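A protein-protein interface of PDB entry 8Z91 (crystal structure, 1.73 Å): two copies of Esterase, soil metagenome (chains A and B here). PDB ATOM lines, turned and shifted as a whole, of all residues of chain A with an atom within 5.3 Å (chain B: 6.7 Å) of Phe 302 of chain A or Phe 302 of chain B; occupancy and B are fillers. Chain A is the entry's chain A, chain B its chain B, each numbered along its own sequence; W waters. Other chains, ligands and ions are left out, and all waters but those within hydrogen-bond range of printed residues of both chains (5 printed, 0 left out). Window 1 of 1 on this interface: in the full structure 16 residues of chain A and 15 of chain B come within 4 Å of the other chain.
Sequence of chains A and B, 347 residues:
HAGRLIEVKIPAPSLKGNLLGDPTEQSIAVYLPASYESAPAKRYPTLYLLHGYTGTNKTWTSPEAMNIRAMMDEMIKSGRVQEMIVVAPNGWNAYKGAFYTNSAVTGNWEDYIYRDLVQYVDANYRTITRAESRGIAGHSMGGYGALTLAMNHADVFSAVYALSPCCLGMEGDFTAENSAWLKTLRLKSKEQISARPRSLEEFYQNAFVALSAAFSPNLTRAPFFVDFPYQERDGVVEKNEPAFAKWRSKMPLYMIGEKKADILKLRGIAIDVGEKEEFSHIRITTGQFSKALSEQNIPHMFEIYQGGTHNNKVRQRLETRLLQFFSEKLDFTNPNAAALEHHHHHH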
ATOM      1  N   ILE A 271      14.840   2.843  -8.131  1.00  0.00           N
ATOM      2  CA  ILE A 271      15.028   2.842  -6.676  1.00  0.00           C
ATOM      3  C   ILE A 271      13.819   3.525  -6.058  1.00  0.00           C
ATOM      4  O   ILE A 271      13.403   4.594  -6.526  1.00  0.00           O
ATOM      5  CB  ILE A 271      16.314   3.594  -6.256  1.00  0.00           C
ATOM      6  CG1 ILE A 271      17.552   3.070  -7.002  1.00  0.00           C
ATOM      7  CG2 ILE A 271      16.479   3.598  -4.724  1.00  0.00           C
ATOM      8  CD1 ILE A 271      18.068   4.056  -8.071  1.00  0.00           C
ATOM      9  N   ASP A 272      13.274   2.959  -4.980  1.00  0.00           N
ATOM     10  CA  ASP A 272      12.203   3.669  -4.288  1.00  0.00           C
ATOM     11  C   ASP A 272      12.376   3.529  -2.776  1.00  0.00           C
ATOM     12  O   ASP A 272      13.231   2.778  -2.278  1.00  0.00           O
ATOM     13  CB  ASP A 272      10.813   3.225  -4.799  1.00  0.00           C
ATOM     14  CG  ASP A 272      10.399   1.801  -4.349  1.00  0.00           C
ATOM     15  OD1 ASP A 272      11.013   1.214  -3.437  1.00  0.00           O
ATOM     16  OD2 ASP A 272       9.426   1.263  -4.931  1.00  0.00           O
ATOM     17  N   VAL A 273      11.583   4.312  -2.054  1.00  0.00           N
ATOM     18  CA  VAL A 273      11.659   4.371  -0.601  1.00  0.00           C
ATOM     19  C   VAL A 273      10.346   4.967  -0.109  1.00  0.00           C
ATOM     20  O   VAL A 273       9.755   5.846  -0.754  1.00  0.00           O
ATOM     21  CB  VAL A 273      12.906   5.161  -0.116  1.00  0.00           C
ATOM     22  CG1 VAL A 273      12.834   6.625  -0.522  1.00  0.00           C
ATOM     23  CG2 VAL A 273      13.082   5.072   1.415  1.00  0.00           C
ATOM     24  N   THR A 286      19.075   6.958  -0.222  1.00  0.00           N
ATOM     25  CA  THR A 286      18.357   6.749  -1.477  1.00  0.00           C
ATOM     26  C   THR A 286      18.214   8.057  -2.249  1.00  0.00           C
ATOM     27  O   THR A 286      18.357   8.079  -3.482  1.00  0.00           O
ATOM     28  CB  THR A 286      16.982   6.115  -1.230  1.00  0.00           C
ATOM     29  OG1 THR A 286      16.229   6.920  -0.315  1.00  0.00           O
ATOM     30  CG2 THR A 286      17.123   4.682  -0.689  1.00  0.00           C
ATOM     31  N   GLY A 287      17.940   9.157  -1.544  1.00  0.00           N
ATOM     32  CA  GLY A 287      17.894  10.456  -2.210  1.00  0.00           C
ATOM     33  C   GLY A 287      19.257  10.862  -2.739  1.00  0.00           C
ATOM     34  O   GLY A 287      19.373  11.402  -3.847  1.00  0.00           O
ATOM     35  N   SER A 290      19.985   8.745  -5.939  1.00  0.00           N
ATOM     36  CA  SER A 290      19.345   9.304  -7.129  1.00  0.00           C
ATOM     37  C   SER A 290      20.028  10.599  -7.575  1.00  0.00           C
ATOM     38  O   SER A 290      20.277  10.789  -8.773  1.00  0.00           O
ATOM     39  CB  SER A 290      17.849   9.525  -6.901  1.00  0.00           C
ATOM     40  OG  SER A 290      17.270  10.102  -8.079  1.00  0.00           O
ATOM     41  N   SER A 294      21.794  11.380 -11.137  1.00  0.00           N
ATOM     42  CA  SER A 294      21.405  12.502 -11.990  1.00  0.00           C
ATOM     43  C   SER A 294      22.578  13.443 -12.249  1.00  0.00           C
ATOM     44  O   SER A 294      22.672  14.016 -13.337  1.00  0.00           O
ATOM     45  CB  SER A 294      20.218  13.267 -11.380  1.00  0.00           C
ATOM     46  OG  SER A 294      20.557  13.885 -10.148  1.00  0.00           O
ATOM     47  N   HIS A 300      17.523   6.670 -15.035  1.00  0.00           N
ATOM     48  CA  HIS A 300      17.026   5.901 -13.893  1.00  0.00           C
ATOM     49  C   HIS A 300      15.663   6.452 -13.478  1.00  0.00           C
ATOM     50  O   HIS A 300      15.255   7.540 -13.899  1.00  0.00           O
ATOM     51  CB  HIS A 300      18.008   5.947 -12.718  1.00  0.00           C
ATOM     52  CG  HIS A 300      17.990   7.243 -11.955  1.00  0.00           C
ATOM     53  ND1 HIS A 300      18.675   8.362 -12.378  1.00  0.00           N
ATOM     54  CD2 HIS A 300      17.429   7.573 -10.767  1.00  0.00           C
ATOM     55  CE1 HIS A 300      18.524   9.330 -11.492  1.00  0.00           C
ATOM     56  NE2 HIS A 300      17.769   8.879 -10.506  1.00  0.00           N
ATOM     57  N   MET A 301      14.986   5.688 -12.622  1.00  0.00           N
ATOM     58  CA  MET A 301      13.691   6.021 -12.046  1.00  0.00           C
ATOM     59  C   MET A 301      13.824   6.070 -10.533  1.00  0.00           C
ATOM     60  O   MET A 301      14.475   5.213  -9.938  1.00  0.00           O
ATOM     61  CB  MET A 301      12.647   4.985 -12.439  1.00  0.00           C
ATOM     62  CG  MET A 301      12.630   4.728 -13.944  1.00  0.00           C
ATOM     63  SD  MET A 301      11.429   3.483 -14.484  1.00  0.00           S
ATOM     64  CE  MET A 301       9.862   4.345 -14.324  1.00  0.00           C
ATOM     65  N   PHE A 302      13.195   7.066  -9.912  1.00  0.00           N
ATOM     66  CA  PHE A 302      13.290   7.244  -8.465  1.00  0.00           C
ATOM     67  C   PHE A 302      11.925   7.652  -7.935  1.00  0.00           C
ATOM     68  O   PHE A 302      11.260   8.510  -8.520  1.00  0.00           O
ATOM     69  CB  PHE A 302      14.338   8.307  -8.111  1.00  0.00           C
ATOM     70  CG  PHE A 302      14.389   8.662  -6.636  1.00  0.00           C
ATOM     71  CD1 PHE A 302      14.702   7.707  -5.678  1.00  0.00           C
ATOM     72  CD2 PHE A 302      14.074   9.944  -6.222  1.00  0.00           C
ATOM     73  CE1 PHE A 302      14.740   8.054  -4.316  1.00  0.00           C
ATOM     74  CE2 PHE A 302      14.107  10.298  -4.876  1.00  0.00           C
ATOM     75  CZ  PHE A 302      14.434   9.361  -3.926  1.00  0.00           C
ATOM     76  N   GLU A 303      11.500   7.048  -6.826  1.00  0.00           N
ATOM     77  CA  GLU A 303      10.238   7.457  -6.210  1.00  0.00           C
ATOM     78  C   GLU A 303      10.326   7.412  -4.692  1.00  0.00           C
ATOM     79  O   GLU A 303      10.833   6.441  -4.125  1.00  0.00           O
ATOM     80  CB  GLU A 303       9.068   6.572  -6.680  1.00  0.00           C
ATOM     81  CG  GLU A 303       7.731   6.981  -6.061  1.00  0.00           C
ATOM     82  CD  GLU A 303       6.551   6.254  -6.665  1.00  0.00           C
ATOM     83  OE1 GLU A 303       6.781   5.355  -7.506  1.00  0.00           O
ATOM     84  OE2 GLU A 303       5.398   6.603  -6.315  1.00  0.00           O
ATOM     85  N   ILE A 304       9.866   8.486  -4.057  1.00  0.00           N
ATOM     86  CA  ILE A 304       9.457   8.486  -2.657  1.00  0.00           C
ATOM     87  C   ILE A 304       7.941   8.368  -2.642  1.00  0.00           C
ATOM     88  O   ILE A 304       7.242   9.246  -3.168  1.00  0.00           O
ATOM     89  CB  ILE A 304       9.920   9.766  -1.942  1.00  0.00           C
ATOM     90  CG1 ILE A 304      11.448   9.926  -2.036  1.00  0.00           C
ATOM     91  CG2 ILE A 304       9.369   9.823  -0.498  1.00  0.00           C
ATOM     92  CD1 ILE A 304      11.948  11.254  -1.418  1.00  0.00           C
ATOM     93  N   ILE B 269       3.081  13.837  -7.691  1.00  0.00           N
ATOM     94  CA  ILE B 269       4.044  14.746  -8.312  1.00  0.00           C
ATOM     95  C   ILE B 269       4.991  13.923  -9.173  1.00  0.00           C
ATOM     96  O   ILE B 269       5.700  13.045  -8.651  1.00  0.00           O
ATOM     97  CB  ILE B 269       4.857  15.529  -7.263  1.00  0.00           C
ATOM     98  CG1 ILE B 269       3.962  16.204  -6.233  1.00  0.00           C
ATOM     99  CG2 ILE B 269       5.815  16.505  -7.933  1.00  0.00           C
ATOM    100  CD1 ILE B 269       4.763  16.843  -5.117  1.00  0.00           C
ATOM    101  N   ALA B 270       5.034  14.208 -10.479  1.00  0.00           N
ATOM    102  CA  ALA B 270       6.006  13.572 -11.370  1.00  0.00           C
ATOM    103  C   ALA B 270       6.771  14.606 -12.196  1.00  0.00           C
ATOM    104  O   ALA B 270       6.198  15.610 -12.643  1.00  0.00           O
ATOM    105  CB  ALA B 270       5.310  12.554 -12.295  1.00  0.00           C
ATOM    106  N   ILE B 271       8.077  14.356 -12.387  1.00  0.00           N
ATOM    107  CA  ILE B 271       8.969  15.188 -13.211  1.00  0.00           C
ATOM    108  C   ILE B 271       9.882  14.279 -14.006  1.00  0.00           C
ATOM    109  O   ILE B 271      10.494  13.358 -13.443  1.00  0.00           O
ATOM    110  CB  ILE B 271       9.851  16.163 -12.395  1.00  0.00           C
ATOM    111  CG1 ILE B 271       9.081  16.867 -11.287  1.00  0.00           C
ATOM    112  CG2 ILE B 271      10.617  17.108 -13.284  1.00  0.00           C
ATOM    113  CD1 ILE B 271       9.536  16.392  -9.898  1.00  0.00           C
ATOM    114  N   ASP B 272       9.994  14.530 -15.309  1.00  0.00           N
ATOM    115  CA  ASP B 272      10.950  13.753 -16.084  1.00  0.00           C
ATOM    116  C   ASP B 272      11.722  14.654 -17.037  1.00  0.00           C
ATOM    117  O   ASP B 272      11.428  15.851 -17.206  1.00  0.00           O
ATOM    118  CB  ASP B 272      10.292  12.545 -16.801  1.00  0.00           C
ATOM    119  CG  ASP B 272       9.345  12.926 -17.940  1.00  0.00           C
ATOM    120  OD1 ASP B 272       9.400  14.047 -18.503  1.00  0.00           O
ATOM    121  OD2 ASP B 272       8.504  12.058 -18.269  1.00  0.00           O
ATOM    122  N   VAL B 273      12.738  14.043 -17.645  1.00  0.00           N
ATOM    123  CA  VAL B 273      13.644  14.739 -18.545  1.00  0.00           C
ATOM    124  C   VAL B 273      14.384  13.678 -19.337  1.00  0.00           C
ATOM    125  O   VAL B 273      14.636  12.572 -18.834  1.00  0.00           O
ATOM    126  CB  VAL B 273      14.615  15.661 -17.764  1.00  0.00           C
ATOM    127  CG1 VAL B 273      15.544  14.859 -16.842  1.00  0.00           C
ATOM    128  CG2 VAL B 273      15.427  16.545 -18.749  1.00  0.00           C
ATOM    129  N   ARG B 283      18.226  20.102 -18.112  1.00  0.00           N
ATOM    130  CA  ARG B 283      18.958  18.933 -17.624  1.00  0.00           C
ATOM    131  C   ARG B 283      19.396  19.132 -16.181  1.00  0.00           C
ATOM    132  O   ARG B 283      19.177  18.269 -15.322  1.00  0.00           O
ATOM    133  CB  ARG B 283      20.171  18.669 -18.522  1.00  0.00           C
ATOM    134  CG  ARG B 283      21.136  17.625 -17.977  1.00  0.00           C
ATOM    135  CD  ARG B 283      22.233  17.321 -18.994  1.00  0.00           C
ATOM    136  NE  ARG B 283      22.886  18.501 -19.561  1.00  0.00           N
ATOM    137  CZ  ARG B 283      23.820  19.218 -18.947  1.00  0.00           C
ATOM    138  NH1 ARG B 283      24.186  18.965 -17.697  1.00  0.00           N
ATOM    139  NH2 ARG B 283      24.415  20.204 -19.608  1.00  0.00           N
ATOM    140  N   THR B 286      16.216  19.946 -13.376  1.00  0.00           N
ATOM    141  CA  THR B 286      15.270  18.862 -13.108  1.00  0.00           C
ATOM    142  C   THR B 286      15.836  17.893 -12.075  1.00  0.00           C
ATOM    143  O   THR B 286      15.128  17.487 -11.151  1.00  0.00           O
ATOM    144  CB  THR B 286      14.899  18.124 -14.399  1.00  0.00           C
ATOM    145  OG1 THR B 286      16.092  17.623 -15.020  1.00  0.00           O
ATOM    146  CG2 THR B 286      14.117  19.069 -15.370  1.00  0.00           C
ATOM    147  N   GLY B 287      17.115  17.534 -12.202  1.00  0.00           N
ATOM    148  CA  GLY B 287      17.770  16.769 -11.144  1.00  0.00           C
ATOM    149  C   GLY B 287      17.853  17.527  -9.827  1.00  0.00           C
ATOM    150  O   GLY B 287      17.690  16.940  -8.749  1.00  0.00           O
ATOM    151  N   GLN B 288      18.154  18.825  -9.885  1.00  0.00           N
ATOM    152  CA  GLN B 288      18.189  19.613  -8.655  1.00  0.00           C
ATOM    153  C   GLN B 288      16.816  19.660  -8.003  1.00  0.00           C
ATOM    154  O   GLN B 288      16.713  19.659  -6.767  1.00  0.00           O
ATOM    155  CB  GLN B 288      18.697  21.027  -8.934  1.00  0.00           C
ATOM    156  CG  GLN B 288      20.183  21.148  -9.261  1.00  0.00           C
ATOM    157  CD  GLN B 288      20.556  22.554  -9.680  1.00  0.00           C
ATOM    158  OE1 GLN B 288      19.755  23.261 -10.307  1.00  0.00           O
ATOM    159  NE2 GLN B 288      21.775  22.975  -9.346  1.00  0.00           N
ATOM    160  N   PHE B 289      15.756  19.673  -8.814  1.00  0.00           N
ATOM    161  CA  PHE B 289      14.409  19.773  -8.266  1.00  0.00           C
ATOM    162  C   PHE B 289      14.025  18.496  -7.530  1.00  0.00           C
ATOM    163  O   PHE B 289      13.454  18.557  -6.435  1.00  0.00           O
ATOM    164  CB  PHE B 289      13.410  20.087  -9.387  1.00  0.00           C
ATOM    165  CG  PHE B 289      12.038  20.489  -8.902  1.00  0.00           C
ATOM    166  CD1 PHE B 289      11.786  21.777  -8.490  1.00  0.00           C
ATOM    167  CD2 PHE B 289      11.006  19.566  -8.861  1.00  0.00           C
ATOM    168  CE1 PHE B 289      10.511  22.150  -8.058  1.00  0.00           C
ATOM    169  CE2 PHE B 289       9.745  19.921  -8.413  1.00  0.00           C
ATOM    170  CZ  PHE B 289       9.498  21.215  -8.021  1.00  0.00           C
ATOM    171  N   SER B 290      14.348  17.322  -8.099  1.00  0.00           N
ATOM    172  CA  SER B 290      14.059  16.076  -7.394  1.00  0.00           C
ATOM    173  C   SER B 290      14.873  15.978  -6.118  1.00  0.00           C
ATOM    174  O   SER B 290      14.377  15.495  -5.092  1.00  0.00           O
ATOM    175  CB  SER B 290      14.337  14.864  -8.292  1.00  0.00           C
ATOM    176  OG  SER B 290      14.001  13.651  -7.624  1.00  0.00           O
ATOM    177  N   LYS B 291      16.134  16.435  -6.158  1.00  0.00           N
ATOM    178  CA  LYS B 291      16.950  16.430  -4.944  1.00  0.00           C
ATOM    179  C   LYS B 291      16.381  17.372  -3.891  1.00  0.00           C
ATOM    180  O   LYS B 291      16.371  17.049  -2.699  1.00  0.00           O
ATOM    181  CB  LYS B 291      18.385  16.818  -5.286  1.00  0.00           C
ATOM    182  CG  LYS B 291      19.265  17.093  -4.082  1.00  0.00           C
ATOM    183  CD  LYS B 291      19.383  15.881  -3.160  1.00  0.00           C
ATOM    184  CE  LYS B 291      19.929  16.314  -1.808  1.00  0.00           C
ATOM    185  NZ  LYS B 291      20.629  15.230  -1.079  1.00  0.00           N
ATOM    186  N   SER B 294      13.490  15.545  -2.393  1.00  0.00           N
ATOM    187  CA  SER B 294      13.847  14.375  -1.601  1.00  0.00           C
ATOM    188  C   SER B 294      14.506  14.779  -0.286  1.00  0.00           C
ATOM    189  O   SER B 294      14.269  14.145   0.743  1.00  0.00           O
ATOM    190  CB  SER B 294      14.723  13.422  -2.426  1.00  0.00           C
ATOM    191  OG  SER B 294      16.066  13.840  -2.503  1.00  0.00           O
ATOM    192  N   HIS B 300       7.293  11.959  -4.422  1.00  0.00           N
ATOM    193  CA  HIS B 300       7.301  12.365  -5.821  1.00  0.00           C
ATOM    194  C   HIS B 300       7.955  11.261  -6.639  1.00  0.00           C
ATOM    195  O   HIS B 300       8.590  10.341  -6.101  1.00  0.00           O
ATOM    196  CB  HIS B 300       8.040  13.696  -6.020  1.00  0.00           C
ATOM    197  CG  HIS B 300       9.533  13.575  -5.940  1.00  0.00           C
ATOM    198  ND1 HIS B 300      10.207  13.492  -4.735  1.00  0.00           N
ATOM    199  CD2 HIS B 300      10.486  13.587  -6.905  1.00  0.00           C
ATOM    200  CE1 HIS B 300      11.511  13.419  -4.968  1.00  0.00           C
ATOM    201  NE2 HIS B 300      11.707  13.465  -6.276  1.00  0.00           N
ATOM    202  N   MET B 301       7.778  11.360  -7.953  1.00  0.00           N
ATOM    203  CA  MET B 301       8.410  10.465  -8.913  1.00  0.00           C
ATOM    204  C   MET B 301       9.323  11.256  -9.837  1.00  0.00           C
ATOM    205  O   MET B 301       8.988  12.371 -10.258  1.00  0.00           O
ATOM    206  CB  MET B 301       7.365   9.707  -9.720  1.00  0.00           C
ATOM    207  CG  MET B 301       6.223   9.172  -8.864  1.00  0.00           C
ATOM    208  SD  MET B 301       4.848   8.490  -9.804  1.00  0.00           S
ATOM    209  CE  MET B 301       5.546   6.963 -10.460  1.00  0.00           C
ATOM    210  N   PHE B 302      10.469  10.669 -10.176  1.00  0.00           N
ATOM    211  CA  PHE B 302      11.465  11.345 -11.000  1.00  0.00           C
ATOM    212  C   PHE B 302      12.078  10.336 -11.966  1.00  0.00           C
ATOM    213  O   PHE B 302      12.415   9.222 -11.566  1.00  0.00           O
ATOM    214  CB  PHE B 302      12.555  11.990 -10.118  1.00  0.00           C
ATOM    215  CG  PHE B 302      13.738  12.562 -10.896  1.00  0.00           C
ATOM    216  CD1 PHE B 302      13.556  13.601 -11.807  1.00  0.00           C
ATOM    217  CD2 PHE B 302      15.022  12.050 -10.706  1.00  0.00           C
ATOM    218  CE1 PHE B 302      14.628  14.124 -12.525  1.00  0.00           C
ATOM    219  CE2 PHE B 302      16.113  12.569 -11.425  1.00  0.00           C
ATOM    220  CZ  PHE B 302      15.909  13.608 -12.328  1.00  0.00           C
ATOM    221  N   GLU B 303      12.252  10.733 -13.224  1.00  0.00           N
ATOM    222  CA  GLU B 303      12.905   9.865 -14.199  1.00  0.00           C
ATOM    223  C   GLU B 303      13.722  10.670 -15.200  1.00  0.00           C
ATOM    224  O   GLU B 303      13.220  11.638 -15.788  1.00  0.00           O
ATOM    225  CB  GLU B 303      11.880   9.019 -14.960  1.00  0.00           C
ATOM    226  CG  GLU B 303      12.548   8.098 -15.985  1.00  0.00           C
ATOM    227  CD  GLU B 303      11.597   7.098 -16.635  1.00  0.00           C
ATOM    228  OE1 GLU B 303      10.363   7.173 -16.414  1.00  0.00           O
ATOM    229  OE2 GLU B 303      12.115   6.200 -17.345  1.00  0.00           O
ATOM    230  N   ILE B 304      14.966  10.247 -15.400  1.00  0.00           N
ATOM    231  CA  ILE B 304      15.745  10.581 -16.594  1.00  0.00           C
ATOM    232  C   ILE B 304      15.605   9.414 -17.567  1.00  0.00           C
ATOM    233  O   ILE B 304      15.977   8.284 -17.238  1.00  0.00           O
ATOM    234  CB  ILE B 304      17.218  10.822 -16.251  1.00  0.00           C
ATOM    235  CG1 ILE B 304      17.359  11.937 -15.218  1.00  0.00           C
ATOM    236  CG2 ILE B 304      18.037  11.083 -17.525  1.00  0.00           C
ATOM    237  CD1 ILE B 304      18.765  12.074 -14.673  1.00  0.00           C
ATOM    238  N   ARG B 317       6.179   9.439 -23.820  1.00  0.00           N
ATOM    239  CA  ARG B 317       5.961   9.738 -22.404  1.00  0.00           C
ATOM    240  C   ARG B 317       4.463   9.848 -22.102  1.00  0.00           C
ATOM    241  O   ARG B 317       3.997   9.388 -21.051  1.00  0.00           O
ATOM    242  CB  ARG B 317       6.676  11.038 -21.996  1.00  0.00           C
ATOM    243  CG  ARG B 317       8.194  11.054 -22.235  1.00  0.00           C
ATOM    244  CD  ARG B 317       8.892   9.864 -21.569  1.00  0.00           C
ATOM    245  NE  ARG B 317       8.907   9.992 -20.109  1.00  0.00           N
ATOM    246  CZ  ARG B 317       9.427   9.074 -19.288  1.00  0.00           C
ATOM    247  NH1 ARG B 317      10.002   7.976 -19.750  1.00  0.00           N
ATOM    248  NH2 ARG B 317       9.361   9.263 -17.972  1.00  0.00           N
HETATM  249  O   HOH W   1      14.839   5.719 -17.035  1.00  0.00           O
HETATM  250  O   HOH W   2      17.310  13.087  -4.730  1.00  0.00           O
HETATM  251  O   HOH W   3      18.358  14.209  -8.657  1.00  0.00           O
HETATM  252  O   HOH W   4      21.297  15.934 -14.720  1.00  0.00           O
HETATM  253  O   HOH W   5      16.551  12.627  -7.345  1.00  0.00           O
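Printed residues of chain B within 4 Å of Phe 302 of chain A: Ser 290 (3.96 Å), Met 301 (3.5 Å) and Phe 302 (2.8 Å).
Printed residues of chain A within 4 Å of Phe 302 of chain B: Ser 290, Met 301 and Phe 302.
Of the printed residues of chain A, Ile 304 of chain B touches Ser 294 (3.8 Å) and His 300 (3.1 Å).
Of the printed residues of chain B, Ser 294 of chain A touches Ile 304 (3.8 Å).
The nearest printed residue of chain B that does not touch Glu 303 of chain A is Phe 302 of chain B (5.0 Å).
O of Ile 304 of chain A is in hydrogen-bond range of N of His 300 of chain B (3.0 Å).
O of Phe 302 of chain B is in hydrogen-bond range of N of Phe 302 of chain A (2.8 Å).
The backbone NH (N) of Ile 304 of chain B lies within hydrogen-bond range of the backbone carbonyl oxygen (O) of His 300 of chain A, 3.1 Å away.
Of the 12 printed residues of chain A, 8 touch a printed residue of chain B.
Of the 19 printed residues of chain B, 7 touch a printed residue of chain A.
Hydrophobic or aromatic side chains of chain B that line the printed part of chain A: Met 301, Phe 302 and Ile 304.
Among the printed residues, 14 pairs touch across the chains.
Among the printed residues, no Asp or Glu carboxylate lies within 4 Å of a Lys or Arg side-chain nitrogen of the other chain.
Ser 290 of chain A touches Phe 302 of chain B, and with the chains exchanged Phe 302 of chain A touches Ser 290 of chain B.
His 300 of chain A touches Ile 304 of chain B, and with the chains exchanged Ile 304 of chain A touches His 300 of chain B.
Met 301 of chain A touches Phe 302 of chain B, and with the chains exchanged Phe 302 of chain A touches Met 301 of chain B.
Met 301 of chain A touches Glu 303 of chain B, and with the chains exchanged Glu 303 of chain A touches Met 301 of chain B.
12 positions are printed for both chains.
Of the 14 pairs that touch across the chains among the printed residues, 13 have their exchanged pair printed and touching as well.
The backbone carbonyl oxygen (O) of Ile 269 of chain B sits at hydrogen-bond distance from the backbone NH (N) of Met 301 of chain B.
The side-chain hydroxyl (OG) of Ser 294 of chain B sits at hydrogen-bond distance from the backbone carbonyl oxygen (O) of Lys 291 of chain B (3.2 Å).
The backbone NH of Ile 271 of chain B lies within hydrogen-bond range of the backbone carbonyl oxygen of Met 301 of chain B, at 3.1 Å.
The backbone NH of Glu 303 of chain B sits at hydrogen-bond distance from the backbone carbonyl oxygen of Ile 271 of chain B.
The side-chain carboxylate (OE1) of Glu 303 of chain B lies within salt-bridge range of the guanidinium group (NH2) of Arg 317 of chain B, at 2.8 Å.
OG of Ser 290 of chain B is in hydrogen-bond range of NE2 of His 300 of chain B, at 2.7 Å.
Gly 287 of chain A touches Ser 294 of chain B.
CD2 of Phe 302 of chain B touches OG of Ser 290 of chain A, at 3.97 Å.
His 300 of chain A touches Glu 303 of chain B.
Met 301 of chain A touches Phe 302 of chain B.
Met 301 of chain A touches Glu 303 of chain B.
OG of Ser 290 of chain B touches CD2 of Phe 302 of chain A (3.96 Å).
CA of Met 301 of chain B touches O of Phe 302 of chain A, at 3.5 Å.
O of His 300 of chain B touches CA of Glu 303 of chain A, 3.3 Å away.
CE of Met 301 of chain B touches OE1 of Glu 303 of chain A, 3.6 Å away.
Ser 294 of chain B touches Ile 304 of chain A (CA to CD1, 3.7 Å).
Water W2 lies within hydrogen-bond range of OG of Ser 294 of chain B (2.7 Å) and O of Gly 287 of chain A (2.8 Å).
Water W3 bridges OG of Ser 294 of chain A (2.7 Å) and O of Gly 287 of chain B (2.8 Å).
Water W5 lies within hydrogen-bond range of the side-chain hydroxyl of Ser 290 of chain A and the side-chain hydroxyl of Ser 290 of chain B.
Water W4 bridges O of Ser 294 of chain A (2.7 Å) and O of Arg 283 of chain B (3.2 Å).
Water W1 lies within hydrogen-bond range of OE2 of Glu 303 of chain B (2.8 Å), O of Ile 304 of chain B (2.8 Å) and N of His 300 of chain A (3.5 Å).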
